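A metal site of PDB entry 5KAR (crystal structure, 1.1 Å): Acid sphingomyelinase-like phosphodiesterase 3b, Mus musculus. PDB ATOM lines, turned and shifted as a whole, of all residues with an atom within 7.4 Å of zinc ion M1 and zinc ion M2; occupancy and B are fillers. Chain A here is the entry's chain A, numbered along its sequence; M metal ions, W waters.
Zinc ion M1 is bound by water W1. Zinc ion M1 is bound by OD1 of Asp 20, at 2.0 Å. NE2 of His 22 is bound to zinc ion M1 (2.1 Å). Zinc ion M1 is bound by a ring nitrogen (NE2) of His 271 (2.1 Å). Zinc ion M1 is bound by the side-chain carboxylate (OD2) of Asp 85 (2.3 Å).
Zinc ion M2 is bound by water W1 (2.0 Å), OD1 of Asn 126 (2.1 Å), NE2 of His 228 (2.1 Å), ND1 of His 269 (2.1 Å) and OD2 of Asp 85 (2.2 Å).
The side-chain amide oxygen of Asn 187 is in hydrogen-bond range of the backbone NH of Asn 126, 3.0 Å away. The side-chain amide oxygen (OD1) of Asn 133 lies within hydrogen-bond range of the side-chain amide nitrogen (ND2) of Asn 126 (2.8 Å). N of Leu 21 lies within hydrogen-bond range of O of Asp 85 (3.2 Å). The backbone carbonyl oxygen (O) of Asp 20 is in hydrogen-bond range of the backbone NH (N) of Thr 296 (3.1 Å). The backbone carbonyl oxygen (O) of Thr 87 is in hydrogen-bond range of a ring nitrogen (ND1) of His 22, at 2.7 Å. OD1 of Asp 85 sits at hydrogen-bond distance from N of His 127 (2.9 Å). The backbone carbonyl oxygen of His 271 is in hydrogen-bond range of the backbone NH of Gly 294 (3.0 Å). The backbone carbonyl oxygen (O) of His 228 is in hydrogen-bond range of the backbone NH (N) of Gly 268.
Of the 27 residues printed, 5 come within 4 Å of zinc ion M1. The nearest printed residue that does not touch zinc ion M1 is His 228 (4.3 Å).
Of the 27 residues printed, 5 come within 4 Å of zinc ion M2.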
ATOM      1  N   SER A  19     -15.377  26.354  -8.034  1.00  0.00           N
ATOM      2  CA  SER A  19     -14.468  26.114  -6.927  1.00  0.00           C
ATOM      3  C   SER A  19     -15.040  25.058  -5.994  1.00  0.00           C
ATOM      4  O   SER A  19     -16.255  24.865  -5.900  1.00  0.00           O
ATOM      5  CB  SER A  19     -14.257  27.400  -6.141  1.00  0.00           C
ATOM      6  OG  SER A  19     -13.062  27.379  -5.390  1.00  0.00           O
ATOM      7  N   ASP A  20     -14.135  24.396  -5.270  1.00  0.00           N
ATOM      8  CA  ASP A  20     -14.499  23.563  -4.144  1.00  0.00           C
ATOM      9  C   ASP A  20     -15.477  22.466  -4.556  1.00  0.00           C
ATOM     10  O   ASP A  20     -16.517  22.279  -3.958  1.00  0.00           O
ATOM     11  CB  ASP A  20     -15.005  24.401  -2.986  1.00  0.00           C
ATOM     12  CG  ASP A  20     -13.905  25.322  -2.459  1.00  0.00           C
ATOM     13  OD1 ASP A  20     -13.181  24.917  -1.531  1.00  0.00           O
ATOM     14  OD2 ASP A  20     -13.782  26.467  -2.934  1.00  0.00           O
ATOM     15  N   LEU A  21     -15.092  21.711  -5.583  1.00  0.00           N
ATOM     16  CA  LEU A  21     -15.869  20.583  -6.058  1.00  0.00           C
ATOM     17  C   LEU A  21     -15.829  19.424  -5.074  1.00  0.00           C
ATOM     18  O   LEU A  21     -16.805  18.683  -4.983  1.00  0.00           O
ATOM     19  CB  LEU A  21     -15.416  20.188  -7.458  1.00  0.00           C
ATOM     20  CG  LEU A  21     -16.047  21.008  -8.592  1.00  0.00           C
ATOM     21  CD1 LEU A  21     -15.916  22.518  -8.460  1.00  0.00           C
ATOM     22  CD2 LEU A  21     -15.524  20.507  -9.947  1.00  0.00           C
ATOM     23  N   HIS A  22     -14.706  19.206  -4.388  1.00  0.00           N
ATOM     24  CA  HIS A  22     -14.527  18.199  -3.344  1.00  0.00           C
ATOM     25  C   HIS A  22     -15.247  16.878  -3.650  1.00  0.00           C
ATOM     26  O   HIS A  22     -16.242  16.526  -3.011  1.00  0.00           O
ATOM     27  CB  HIS A  22     -15.018  18.717  -1.983  1.00  0.00           C
ATOM     28  CG  HIS A  22     -14.192  19.803  -1.369  1.00  0.00           C
ATOM     29  ND1 HIS A  22     -12.964  19.578  -0.780  1.00  0.00           N
ATOM     30  CD2 HIS A  22     -14.450  21.113  -1.182  1.00  0.00           C
ATOM     31  CE1 HIS A  22     -12.500  20.711  -0.274  1.00  0.00           C
ATOM     32  NE2 HIS A  22     -13.367  21.669  -0.516  1.00  0.00           N
ATOM     33  N   ASP A  57     -19.413  15.373   1.062  1.00  0.00           N
ATOM     34  CA  ASP A  57     -18.834  15.960  -0.130  1.00  0.00           C
ATOM     35  C   ASP A  57     -19.469  15.355  -1.400  1.00  0.00           C
ATOM     36  O   ASP A  57     -20.315  14.459  -1.342  1.00  0.00           O
ATOM     37  CB  ASP A  57     -17.312  15.790  -0.103  1.00  0.00           C
ATOM     38  CG  ASP A  57     -16.618  16.854   0.712  1.00  0.00           C
ATOM     39  OD1 ASP A  57     -16.959  18.059   0.586  1.00  0.00           O
ATOM     40  OD2 ASP A  57     -15.703  16.470   1.472  1.00  0.00           O
ATOM     41  N   THR A  83     -10.697  27.401  -8.979  1.00  0.00           N
ATOM     42  CA  THR A  83      -9.848  27.699  -7.829  1.00  0.00           C
ATOM     43  C   THR A  83      -9.728  26.551  -6.827  1.00  0.00           C
ATOM     44  O   THR A  83      -9.468  26.802  -5.654  1.00  0.00           O
ATOM     45  CB  THR A  83     -10.248  29.039  -7.205  1.00  0.00           C
ATOM     46  OG1 THR A  83     -11.653  29.092  -6.952  1.00  0.00           O
ATOM     47  CG2 THR A  83      -9.941  30.181  -8.119  1.00  0.00           C
ATOM     48  N   GLY A  84      -9.895  25.291  -7.258  1.00  0.00           N
ATOM     49  CA  GLY A  84      -9.347  24.163  -6.540  1.00  0.00           C
ATOM     50  C   GLY A  84     -10.220  23.605  -5.444  1.00  0.00           C
ATOM     51  O   GLY A  84     -11.376  23.981  -5.251  1.00  0.00           O
ATOM     52  N   ASP A  85      -9.608  22.683  -4.700  1.00  0.00           N
ATOM     53  CA  ASP A  85     -10.198  21.873  -3.616  1.00  0.00           C
ATOM     54  C   ASP A  85     -11.050  20.752  -4.197  1.00  0.00           C
ATOM     55  O   ASP A  85     -12.286  20.827  -4.255  1.00  0.00           O
ATOM     56  CB  ASP A  85     -10.969  22.707  -2.598  1.00  0.00           C
ATOM     57  CG  ASP A  85     -10.212  22.962  -1.309  1.00  0.00           C
ATOM     58  OD1 ASP A  85      -9.012  22.673  -1.247  1.00  0.00           O
ATOM     59  OD2 ASP A  85     -10.875  23.453  -0.354  1.00  0.00           O
ATOM     60  N   ASP A  86     -10.382  19.670  -4.576  1.00  0.00           N
ATOM     61  CA  ASP A  86     -10.955  18.616  -5.381  1.00  0.00           C
ATOM     62  C   ASP A  86     -11.225  17.332  -4.627  1.00  0.00           C
ATOM     63  O   ASP A  86     -11.920  16.435  -5.163  1.00  0.00           O
ATOM     64  CB  ASP A  86     -10.010  18.260  -6.535  1.00  0.00           C
ATOM     65  CG  ASP A  86      -9.631  19.456  -7.392  1.00  0.00           C
ATOM     66  OD1 ASP A  86     -10.335  20.475  -7.386  1.00  0.00           O
ATOM     67  OD2 ASP A  86      -8.611  19.313  -8.119  1.00  0.00           O
ATOM     68  N   THR A  87     -10.645  17.170  -3.445  1.00  0.00           N
ATOM     69  CA  THR A  87     -10.619  15.929  -2.703  1.00  0.00           C
ATOM     70  C   THR A  87     -11.505  16.062  -1.478  1.00  0.00           C
ATOM     71  O   THR A  87     -11.912  17.155  -1.089  1.00  0.00           O
ATOM     72  CB  THR A  87      -9.177  15.659  -2.262  1.00  0.00           C
ATOM     73  OG1 THR A  87      -8.804  16.739  -1.425  1.00  0.00           O
ATOM     74  CG2 THR A  87      -8.218  15.583  -3.441  1.00  0.00           C
ATOM     75  N   HIS A  89     -13.132  15.734   2.508  1.00  0.00           N
ATOM     76  CA  HIS A  89     -12.774  16.070   3.879  1.00  0.00           C
ATOM     77  C   HIS A  89     -12.736  14.782   4.694  1.00  0.00           C
ATOM     78  O   HIS A  89     -13.723  14.381   5.323  1.00  0.00           O
ATOM     79  CB  HIS A  89     -13.783  17.039   4.468  1.00  0.00           C
ATOM     80  CG  HIS A  89     -13.835  18.362   3.782  1.00  0.00           C
ATOM     81  ND1 HIS A  89     -14.575  18.565   2.649  1.00  0.00           N
ATOM     82  CD2 HIS A  89     -13.225  19.544   4.053  1.00  0.00           C
ATOM     83  CE1 HIS A  89     -14.456  19.826   2.258  1.00  0.00           C
ATOM     84  NE2 HIS A  89     -13.638  20.429   3.080  1.00  0.00           N
ATOM     85  N   GLY A 125      -6.132  24.128  -4.459  1.00  0.00           N
ATOM     86  CA  GLY A 125      -6.701  24.389  -3.166  1.00  0.00           C
ATOM     87  C   GLY A 125      -5.994  23.613  -2.070  1.00  0.00           C
ATOM     88  O   GLY A 125      -5.196  22.722  -2.330  1.00  0.00           O
ATOM     89  N   ASN A 126      -6.344  23.940  -0.820  1.00  0.00           N
ATOM     90  CA  ASN A 126      -5.578  23.428   0.313  1.00  0.00           C
ATOM     91  C   ASN A 126      -5.725  21.917   0.488  1.00  0.00           C
ATOM     92  O   ASN A 126      -4.820  21.286   1.065  1.00  0.00           O
ATOM     93  CB  ASN A 126      -5.915  24.198   1.593  1.00  0.00           C
ATOM     94  CG  ASN A 126      -7.386  24.119   1.958  1.00  0.00           C
ATOM     95  OD1 ASN A 126      -8.225  24.603   1.233  1.00  0.00           O
ATOM     96  ND2 ASN A 126      -7.704  23.504   3.101  1.00  0.00           N
ATOM     97  N   HIS A 127      -6.810  21.344   0.002  1.00  0.00           N
ATOM     98  CA  HIS A 127      -7.004  19.900   0.023  1.00  0.00           C
ATOM     99  C   HIS A 127      -6.367  19.189  -1.152  1.00  0.00           C
ATOM    100  O   HIS A 127      -6.363  17.934  -1.172  1.00  0.00           O
ATOM    101  CB  HIS A 127      -8.497  19.585   0.053  1.00  0.00           C
ATOM    102  CG  HIS A 127      -9.116  19.853   1.375  1.00  0.00           C
ATOM    103  ND1 HIS A 127      -9.181  18.913   2.376  1.00  0.00           N
ATOM    104  CD2 HIS A 127      -9.627  20.987   1.898  1.00  0.00           C
ATOM    105  CE1 HIS A 127      -9.726  19.444   3.449  1.00  0.00           C
ATOM    106  NE2 HIS A 127      -9.996  20.712   3.198  1.00  0.00           N
ATOM    107  N   ASN A 133      -3.077  20.618   3.275  1.00  0.00           N
ATOM    108  CA  ASN A 133      -2.656  21.931   3.713  1.00  0.00           C
ATOM    109  C   ASN A 133      -1.145  22.115   3.719  1.00  0.00           C
ATOM    110  O   ASN A 133      -0.706  23.224   3.902  1.00  0.00           O
ATOM    111  CB  ASN A 133      -3.199  22.323   5.106  1.00  0.00           C
ATOM    112  CG  ASN A 133      -4.683  22.159   5.198  1.00  0.00           C
ATOM    113  OD1 ASN A 133      -5.404  22.466   4.251  1.00  0.00           O
ATOM    114  ND2 ASN A 133      -5.143  21.622   6.306  1.00  0.00           N
ATOM    115  N   ASN A 187      -2.298  28.759  -0.501  1.00  0.00           N
ATOM    116  CA  ASN A 187      -2.130  27.710   0.504  1.00  0.00           C
ATOM    117  C   ASN A 187      -0.810  27.858   1.237  1.00  0.00           C
ATOM    118  O   ASN A 187      -0.676  27.350   2.359  1.00  0.00           O
ATOM    119  CB  ASN A 187      -2.252  26.346  -0.180  1.00  0.00           C
ATOM    120  CG  ASN A 187      -3.455  26.278  -1.092  1.00  0.00           C
ATOM    121  OD1 ASN A 187      -4.594  26.395  -0.644  1.00  0.00           O
ATOM    122  ND2 ASN A 187      -3.208  26.168  -2.366  1.00  0.00           N
ATOM    123  N   TYR A 190      -1.673  29.626   4.687  1.00  0.00           N
ATOM    124  CA  TYR A 190      -2.598  29.087   5.661  1.00  0.00           C
ATOM    125  C   TYR A 190      -1.856  28.776   6.967  1.00  0.00           C
ATOM    126  O   TYR A 190      -0.777  28.190   6.972  1.00  0.00           O
ATOM    127  CB  TYR A 190      -3.257  27.836   5.046  1.00  0.00           C
ATOM    128  CG  TYR A 190      -4.437  27.215   5.761  1.00  0.00           C
ATOM    129  CD1 TYR A 190      -5.061  27.804   6.871  1.00  0.00           C
ATOM    130  CD2 TYR A 190      -4.905  25.977   5.366  1.00  0.00           C
ATOM    131  CE1 TYR A 190      -6.126  27.190   7.514  1.00  0.00           C
ATOM    132  CE2 TYR A 190      -5.949  25.373   6.001  1.00  0.00           C
ATOM    133  CZ  TYR A 190      -6.550  25.971   7.064  1.00  0.00           C
ATOM    134  OH  TYR A 190      -7.607  25.319   7.689  1.00  0.00           O
ATOM    135  N   HIS A 228      -7.083  30.250  -4.006  1.00  0.00           N
ATOM    136  CA  HIS A 228      -8.010  29.420  -3.256  1.00  0.00           C
ATOM    137  C   HIS A 228      -8.352  30.043  -1.905  1.00  0.00           C
ATOM    138  O   HIS A 228      -9.507  30.436  -1.698  1.00  0.00           O
ATOM    139  CB  HIS A 228      -7.488  28.005  -3.068  1.00  0.00           C
ATOM    140  CG  HIS A 228      -8.446  27.157  -2.323  1.00  0.00           C
ATOM    141  ND1 HIS A 228      -9.615  26.723  -2.909  1.00  0.00           N
ATOM    142  CD2 HIS A 228      -8.491  26.780  -1.032  1.00  0.00           C
ATOM    143  CE1 HIS A 228     -10.325  26.062  -2.007  1.00  0.00           C
ATOM    144  NE2 HIS A 228      -9.660  26.067  -0.867  1.00  0.00           N
ATOM    145  N   VAL A 229      -7.392  30.093  -0.981  1.00  0.00           N
ATOM    146  CA  VAL A 229      -7.612  30.604   0.376  1.00  0.00           C
ATOM    147  C   VAL A 229      -7.590  32.129   0.319  1.00  0.00           C
ATOM    148  O   VAL A 229      -6.578  32.707  -0.130  1.00  0.00           O
ATOM    149  CB  VAL A 229      -6.526  30.096   1.338  1.00  0.00           C
ATOM    150  CG1 VAL A 229      -6.810  30.609   2.752  1.00  0.00           C
ATOM    151  CG2 VAL A 229      -6.434  28.574   1.342  1.00  0.00           C
ATOM    152  N   PRO A 230      -8.608  32.809   0.828  1.00  0.00           N
ATOM    153  CA  PRO A 230      -8.602  34.286   0.812  1.00  0.00           C
ATOM    154  C   PRO A 230      -7.959  34.845   2.052  1.00  0.00           C
ATOM    155  O   PRO A 230      -7.915  34.165   3.093  1.00  0.00           O
ATOM    156  CB  PRO A 230     -10.092  34.622   0.810  1.00  0.00           C
ATOM    157  CG  PRO A 230     -10.691  33.524   1.611  1.00  0.00           C
ATOM    158  CD  PRO A 230      -9.918  32.274   1.266  1.00  0.00           C
ATOM    159  N   GLY A 268     -12.078  31.157  -3.350  1.00  0.00           N
ATOM    160  CA  GLY A 268     -13.023  30.147  -2.913  1.00  0.00           C
ATOM    161  C   GLY A 268     -12.824  29.816  -1.433  1.00  0.00           C
ATOM    162  O   GLY A 268     -12.743  30.747  -0.615  1.00  0.00           O
ATOM    163  N   HIS A 269     -12.700  28.524  -1.114  1.00  0.00           N
ATOM    164  CA  HIS A 269     -12.378  27.984   0.199  1.00  0.00           C
ATOM    165  C   HIS A 269     -13.511  28.016   1.203  1.00  0.00           C
ATOM    166  O   HIS A 269     -13.686  27.045   1.945  1.00  0.00           O
ATOM    167  CB  HIS A 269     -11.108  28.654   0.747  1.00  0.00           C
ATOM    168  CG  HIS A 269     -10.626  28.086   2.045  1.00  0.00           C
ATOM    169  ND1 HIS A 269     -10.214  26.779   2.196  1.00  0.00           N
ATOM    170  CD2 HIS A 269     -10.543  28.667   3.263  1.00  0.00           C
ATOM    171  CE1 HIS A 269      -9.851  26.596   3.451  1.00  0.00           C
ATOM    172  NE2 HIS A 269     -10.028  27.728   4.119  1.00  0.00           N
ATOM    173  N   HIS A 270     -14.314  29.060   1.218  1.00  0.00           N
ATOM    174  CA  HIS A 270     -15.381  29.163   2.200  1.00  0.00           C
ATOM    175  C   HIS A 270     -16.569  28.269   1.867  1.00  0.00           C
ATOM    176  O   HIS A 270     -17.270  27.860   2.780  1.00  0.00           O
ATOM    177  CB  HIS A 270     -15.868  30.577   2.301  1.00  0.00           C
ATOM    178  CG  HIS A 270     -14.878  31.479   2.960  1.00  0.00           C
ATOM    179  ND1 HIS A 270     -15.022  32.850   2.962  1.00  0.00           N
ATOM    180  CD2 HIS A 270     -13.748  31.219   3.647  1.00  0.00           C
ATOM    181  CE1 HIS A 270     -14.019  33.391   3.630  1.00  0.00           C
ATOM    182  NE2 HIS A 270     -13.221  32.433   4.042  1.00  0.00           N
ATOM    183  N   HIS A 271     -16.842  28.059   0.599  1.00  0.00           N
ATOM    184  CA  HIS A 271     -17.984  27.331   0.037  1.00  0.00           C
ATOM    185  C   HIS A 271     -19.245  28.165   0.030  1.00  0.00           C
ATOM    186  O   HIS A 271     -20.252  27.750  -0.552  1.00  0.00           O
ATOM    187  CB  HIS A 271     -18.275  25.976   0.694  1.00  0.00           C
ATOM    188  CG  HIS A 271     -17.102  25.063   0.720  1.00  0.00           C
ATOM    189  ND1 HIS A 271     -17.149  23.827   1.315  1.00  0.00           N
ATOM    190  CD2 HIS A 271     -15.841  25.200   0.239  1.00  0.00           C
ATOM    191  CE1 HIS A 271     -15.963  23.240   1.193  1.00  0.00           C
ATOM    192  NE2 HIS A 271     -15.143  24.056   0.545  1.00  0.00           N
ATOM    193  N   GLY A 294     -19.227  26.879  -3.247  1.00  0.00           N
ATOM    194  CA  GLY A 294     -18.730  25.602  -3.718  1.00  0.00           C
ATOM    195  C   GLY A 294     -19.786  24.759  -4.390  1.00  0.00           C
ATOM    196  O   GLY A 294     -20.987  24.941  -4.188  1.00  0.00           O
ATOM    197  N   THR A 296     -19.525  21.462  -3.733  1.00  0.00           N
ATOM    198  CA  THR A 296     -19.823  20.557  -2.627  1.00  0.00           C
ATOM    199  C   THR A 296     -20.835  21.208  -1.684  1.00  0.00           C
ATOM    200  O   THR A 296     -20.745  22.414  -1.412  1.00  0.00           O
ATOM    201  CB  THR A 296     -18.568  20.159  -1.857  1.00  0.00           C
ATOM    202  OG1 THR A 296     -18.928  19.066  -1.009  1.00  0.00           O
ATOM    203  CG2 THR A 296     -18.001  21.285  -1.007  1.00  0.00           C
ATOM    204  N   TRP A 298     -21.259  20.048   1.478  1.00  0.00           N
ATOM    205  CA  TRP A 298     -20.796  19.485   2.755  1.00  0.00           C
ATOM    206  C   TRP A 298     -20.974  20.427   3.946  1.00  0.00           C
ATOM    207  O   TRP A 298     -20.447  21.542   3.973  1.00  0.00           O
ATOM    208  CB  TRP A 298     -19.314  19.169   2.565  1.00  0.00           C
ATOM    209  CG  TRP A 298     -18.551  18.641   3.726  1.00  0.00           C
ATOM    210  CD1 TRP A 298     -18.563  17.387   4.197  1.00  0.00           C
ATOM    211  CD2 TRP A 298     -17.612  19.357   4.507  1.00  0.00           C
ATOM    212  NE1 TRP A 298     -17.703  17.262   5.262  1.00  0.00           N
ATOM    213  CE2 TRP A 298     -17.098  18.466   5.476  1.00  0.00           C
ATOM    214  CE3 TRP A 298     -17.146  20.670   4.488  1.00  0.00           C
ATOM    215  CZ2 TRP A 298     -16.142  18.844   6.404  1.00  0.00           C
ATOM    216  CZ3 TRP A 298     -16.191  21.038   5.414  1.00  0.00           C
ATOM    217  CH2 TRP A 298     -15.708  20.132   6.367  1.00  0.00           C
HETATM  218 ZN    ZN M   1     -13.161  23.638   0.041  1.00  0.00          ZN
HETATM  219 ZN    ZN M   2     -10.210  25.082   0.901  1.00  0.00          ZN
HETATM  220  O   HOH W   1     -12.163  24.688   1.364  1.00  0.00           O
